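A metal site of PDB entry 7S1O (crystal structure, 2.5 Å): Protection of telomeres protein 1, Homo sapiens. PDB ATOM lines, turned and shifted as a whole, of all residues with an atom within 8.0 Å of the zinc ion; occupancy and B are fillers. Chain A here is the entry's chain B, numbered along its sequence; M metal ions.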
ATOM      1  N   HIS A  60       7.015  31.011 -26.973  1.00  0.00           N
ATOM      2  CA  HIS A  60       7.243  30.605 -25.590  1.00  0.00           C
ATOM      3  C   HIS A  60       6.144  31.118 -24.680  1.00  0.00           C
ATOM      4  O   HIS A  60       5.769  32.292 -24.747  1.00  0.00           O
ATOM      5  CB  HIS A  60       8.599  31.091 -25.089  1.00  0.00           C
ATOM      6  CG  HIS A  60       8.755  30.985 -23.596  1.00  0.00           C
ATOM      7  ND1 HIS A  60       8.754  32.095 -22.774  1.00  0.00           N
ATOM      8  CD2 HIS A  60       8.902  29.913 -22.792  1.00  0.00           C
ATOM      9  CE1 HIS A  60       8.907  31.700 -21.524  1.00  0.00           C
ATOM     10  NE2 HIS A  60       8.997  30.373 -21.506  1.00  0.00           N
ATOM     11  N   CYS A  61       5.667  30.240 -23.806  1.00  0.00           N
ATOM     12  CA  CYS A  61       4.682  30.596 -22.816  1.00  0.00           C
ATOM     13  C   CYS A  61       5.369  31.249 -21.614  1.00  0.00           C
ATOM     14  O   CYS A  61       6.223  30.607 -20.985  1.00  0.00           O
ATOM     15  CB  CYS A  61       3.930  29.361 -22.374  1.00  0.00           C
ATOM     16  SG  CYS A  61       2.388  29.154 -23.201  1.00  0.00           S
ATOM     17  N   PRO A  62       5.039  32.499 -21.263  1.00  0.00           N
ATOM     18  CA  PRO A  62       5.628  33.070 -20.048  1.00  0.00           C
ATOM     19  C   PRO A  62       5.152  32.384 -18.777  1.00  0.00           C
ATOM     20  O   PRO A  62       5.793  32.530 -17.730  1.00  0.00           O
ATOM     21  CB  PRO A  62       5.171  34.533 -20.102  1.00  0.00           C
ATOM     22  CG  PRO A  62       3.889  34.484 -20.867  1.00  0.00           C
ATOM     23  CD  PRO A  62       4.070  33.398 -21.900  1.00  0.00           C
ATOM     24  N   LYS A  63       4.056  31.614 -18.837  1.00  0.00           N
ATOM     25  CA  LYS A  63       3.450  30.954 -17.695  1.00  0.00           C
ATOM     26  C   LYS A  63       3.643  29.453 -17.713  1.00  0.00           C
ATOM     27  O   LYS A  63       4.146  28.864 -16.744  1.00  0.00           O
ATOM     28  CB  LYS A  63       1.957  31.295 -17.642  1.00  0.00           C
ATOM     29  CG  LYS A  63       1.102  30.360 -16.819  1.00  0.00           C
ATOM     30  CD  LYS A  63      -0.371  30.670 -17.041  1.00  0.00           C
ATOM     31  CE  LYS A  63      -1.123  30.751 -15.732  1.00  0.00           C
ATOM     32  NZ  LYS A  63      -2.538  31.189 -15.926  1.00  0.00           N
ATOM     33  N   CYS A  64       3.254  28.793 -18.812  1.00  0.00           N
ATOM     34  CA  CYS A  64       3.444  27.353 -18.924  1.00  0.00           C
ATOM     35  C   CYS A  64       4.908  26.994 -19.079  1.00  0.00           C
ATOM     36  O   CYS A  64       5.355  25.942 -18.597  1.00  0.00           O
ATOM     37  CB  CYS A  64       2.643  26.810 -20.104  1.00  0.00           C
ATOM     38  SG  CYS A  64       2.740  25.023 -20.349  1.00  0.00           S
ATOM     39  N   HIS A  65       5.678  27.857 -19.749  1.00  0.00           N
ATOM     40  CA  HIS A  65       7.047  27.638 -20.208  1.00  0.00           C
ATOM     41  C   HIS A  65       7.124  26.645 -21.360  1.00  0.00           C
ATOM     42  O   HIS A  65       8.219  26.177 -21.710  1.00  0.00           O
ATOM     43  CB  HIS A  65       7.974  27.185 -19.069  1.00  0.00           C
ATOM     44  CG  HIS A  65       8.095  28.178 -17.966  1.00  0.00           C
ATOM     45  ND1 HIS A  65       8.430  29.492 -18.179  1.00  0.00           N
ATOM     46  CD2 HIS A  65       7.940  28.049 -16.620  1.00  0.00           C
ATOM     47  CE1 HIS A  65       8.467  30.143 -17.030  1.00  0.00           C
ATOM     48  NE2 HIS A  65       8.176  29.281 -16.063  1.00  0.00           N
ATOM     49  N   LEU A  66       5.990  26.323 -21.985  1.00  0.00           N
ATOM     50  CA  LEU A  66       5.989  25.456 -23.147  1.00  0.00           C
ATOM     51  C   LEU A  66       6.591  26.171 -24.353  1.00  0.00           C
ATOM     52  O   LEU A  66       6.462  27.392 -24.507  1.00  0.00           O
ATOM     53  CB  LEU A  66       4.559  25.000 -23.471  1.00  0.00           C
ATOM     54  CG  LEU A  66       4.192  24.614 -24.903  1.00  0.00           C
ATOM     55  CD1 LEU A  66       4.628  23.184 -25.217  1.00  0.00           C
ATOM     56  CD2 LEU A  66       2.695  24.792 -25.143  1.00  0.00           C
ATOM     57  N   LEU A  67       7.260  25.412 -25.206  1.00  0.00           N
ATOM     58  CA  LEU A  67       7.803  25.927 -26.461  1.00  0.00           C
ATOM     59  C   LEU A  67       6.999  25.355 -27.621  1.00  0.00           C
ATOM     60  O   LEU A  67       6.839  24.133 -27.732  1.00  0.00           O
ATOM     61  CB  LEU A  67       9.292  25.585 -26.608  1.00  0.00           C
ATOM     62  CG  LEU A  67      10.245  26.368 -25.706  1.00  0.00           C
ATOM     63  CD1 LEU A  67      11.675  25.890 -25.902  1.00  0.00           C
ATOM     64  CD2 LEU A  67      10.134  27.859 -25.986  1.00  0.00           C
ATOM     65  N   GLN A  68       6.496  26.238 -28.472  1.00  0.00           N
ATOM     66  CA  GLN A  68       5.734  25.855 -29.649  1.00  0.00           C
ATOM     67  C   GLN A  68       6.407  26.385 -30.900  1.00  0.00           C
ATOM     68  O   GLN A  68       7.201  27.328 -30.857  1.00  0.00           O
ATOM     69  CB  GLN A  68       4.287  26.386 -29.571  1.00  0.00           C
ATOM     70  CG  GLN A  68       3.292  25.571 -30.361  1.00  0.00           C
ATOM     71  CD  GLN A  68       2.667  24.463 -29.551  1.00  0.00           C
ATOM     72  OE1 GLN A  68       2.180  24.692 -28.437  1.00  0.00           O
ATOM     73  NE2 GLN A  68       2.647  23.256 -30.100  1.00  0.00           N
ATOM     74  N   GLY A 181      -1.706  32.684 -28.917  1.00  0.00           N
ATOM     75  CA  GLY A 181      -1.951  32.432 -27.515  1.00  0.00           C
ATOM     76  C   GLY A 181      -1.723  30.991 -27.119  1.00  0.00           C
ATOM     77  O   GLY A 181      -1.679  30.099 -27.979  1.00  0.00           O
ATOM     78  N   CYS A 182      -1.565  30.747 -25.815  1.00  0.00           N
ATOM     79  CA  CYS A 182      -1.370  29.397 -25.312  1.00  0.00           C
ATOM     80  C   CYS A 182      -2.663  28.584 -25.365  1.00  0.00           C
ATOM     81  O   CYS A 182      -3.676  28.987 -24.775  1.00  0.00           O
ATOM     82  CB  CYS A 182      -0.862  29.443 -23.877  1.00  0.00           C
ATOM     83  SG  CYS A 182      -0.674  27.804 -23.142  1.00  0.00           S
ATOM     84  N   LYS A 183      -2.620  27.431 -26.031  1.00  0.00           N
ATOM     85  CA  LYS A 183      -3.788  26.575 -26.091  1.00  0.00           C
ATOM     86  C   LYS A 183      -4.102  25.894 -24.766  1.00  0.00           C
ATOM     87  O   LYS A 183      -5.166  25.287 -24.639  1.00  0.00           O
ATOM     88  CB  LYS A 183      -3.614  25.507 -27.188  1.00  0.00           C
ATOM     89  CG  LYS A 183      -2.878  25.995 -28.411  1.00  0.00           C
ATOM     90  CD  LYS A 183      -2.579  24.837 -29.360  1.00  0.00           C
ATOM     91  CE  LYS A 183      -3.852  24.287 -29.974  1.00  0.00           C
ATOM     92  NZ  LYS A 183      -3.643  23.823 -31.374  1.00  0.00           N
ATOM     93  N   GLN A 184      -3.202  25.983 -23.783  1.00  0.00           N
ATOM     94  CA  GLN A 184      -3.383  25.323 -22.493  1.00  0.00           C
ATOM     95  C   GLN A 184      -3.744  26.299 -21.376  1.00  0.00           C
ATOM     96  O   GLN A 184      -4.686  26.058 -20.610  1.00  0.00           O
ATOM     97  CB  GLN A 184      -2.107  24.554 -22.113  1.00  0.00           C
ATOM     98  CG  GLN A 184      -1.744  23.439 -23.075  1.00  0.00           C
ATOM     99  CD  GLN A 184      -2.542  22.180 -22.833  1.00  0.00           C
ATOM    100  OE1 GLN A 184      -3.393  21.794 -23.630  1.00  0.00           O
ATOM    101  NE2 GLN A 184      -2.280  21.524 -21.712  1.00  0.00           N
ATOM    102  N   CYS A 185      -3.024  27.412 -21.269  1.00  0.00           N
ATOM    103  CA  CYS A 185      -3.210  28.364 -20.188  1.00  0.00           C
ATOM    104  C   CYS A 185      -4.368  29.327 -20.409  1.00  0.00           C
ATOM    105  O   CYS A 185      -4.691  30.104 -19.503  1.00  0.00           O
ATOM    106  CB  CYS A 185      -1.914  29.166 -19.980  1.00  0.00           C
ATOM    107  SG  CYS A 185      -0.489  28.120 -19.677  1.00  0.00           S
ATOM    108  N   SER A 186      -4.988  29.295 -21.574  1.00  0.00           N
ATOM    109  CA  SER A 186      -6.009  30.271 -21.923  1.00  0.00           C
ATOM    110  C   SER A 186      -7.399  29.672 -21.740  1.00  0.00           C
ATOM    111  O   SER A 186      -7.619  28.477 -21.940  1.00  0.00           O
ATOM    112  CB  SER A 186      -5.838  30.742 -23.363  1.00  0.00           C
ATOM    113  OG  SER A 186      -4.758  31.650 -23.461  1.00  0.00           O
ATOM    114  N   VAL A 215      -3.617  33.973 -22.819  1.00  0.00           N
ATOM    115  CA  VAL A 215      -2.225  34.156 -22.405  1.00  0.00           C
ATOM    116  C   VAL A 215      -1.377  34.185 -23.677  1.00  0.00           C
ATOM    117  O   VAL A 215      -1.224  33.138 -24.333  1.00  0.00           O
ATOM    118  CB  VAL A 215      -1.756  33.036 -21.463  1.00  0.00           C
ATOM    119  CG1 VAL A 215      -0.501  33.480 -20.710  1.00  0.00           C
ATOM    120  CG2 VAL A 215      -2.868  32.673 -20.485  1.00  0.00           C
ATOM    121  N   PRO A 216      -0.822  35.329 -24.060  1.00  0.00           N
ATOM    122  CA  PRO A 216      -0.131  35.418 -25.353  1.00  0.00           C
ATOM    123  C   PRO A 216       1.257  34.791 -25.304  1.00  0.00           C
ATOM    124  O   PRO A 216       1.990  34.932 -24.324  1.00  0.00           O
ATOM    125  CB  PRO A 216      -0.030  36.934 -25.606  1.00  0.00           C
ATOM    126  CG  PRO A 216      -0.698  37.606 -24.422  1.00  0.00           C
ATOM    127  CD  PRO A 216      -0.780  36.606 -23.327  1.00  0.00           C
ATOM    128  N   LEU A 217       1.602  34.099 -26.379  1.00  0.00           N
ATOM    129  CA  LEU A 217       2.942  33.562 -26.518  1.00  0.00           C
ATOM    130  C   LEU A 217       3.926  34.691 -26.815  1.00  0.00           C
ATOM    131  O   LEU A 217       3.541  35.831 -27.103  1.00  0.00           O
ATOM    132  CB  LEU A 217       2.999  32.510 -27.625  1.00  0.00           C
ATOM    133  CG  LEU A 217       1.911  31.430 -27.532  1.00  0.00           C
ATOM    134  CD1 LEU A 217       2.101  30.372 -28.613  1.00  0.00           C
ATOM    135  CD2 LEU A 217       1.909  30.807 -26.161  1.00  0.00           C
HETATM  136 ZN    ZN M   1       0.891  28.249 -21.507  1.00  0.00          ZN
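The side-chain sulfur of Cys 182 lies close to the backbone NH of Gln 184, at 3.2 Å.
N of Cys 182 sits at hydrogen-bond distance from O of Val 215, 2.8 Å away.
The backbone carbonyl oxygen (O) of Cys 182 lies close to the side-chain hydroxyl (OG) of Ser 186.
The backbone carbonyl oxygen (O) of Leu 66 is in hydrogen-bond range of the backbone NH (N) of Cys 61 (3.0 Å).
The zinc ion is bound by SG of Cys 185 (2.3 Å), SG of Cys 182 (2.3 Å) and SG of Cys 61 (2.4 Å).
Cys 64 touches the zinc ion.
Within 4 Å of the zinc ion: Cys 61, Cys 64, Cys 182 and Cys 185.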
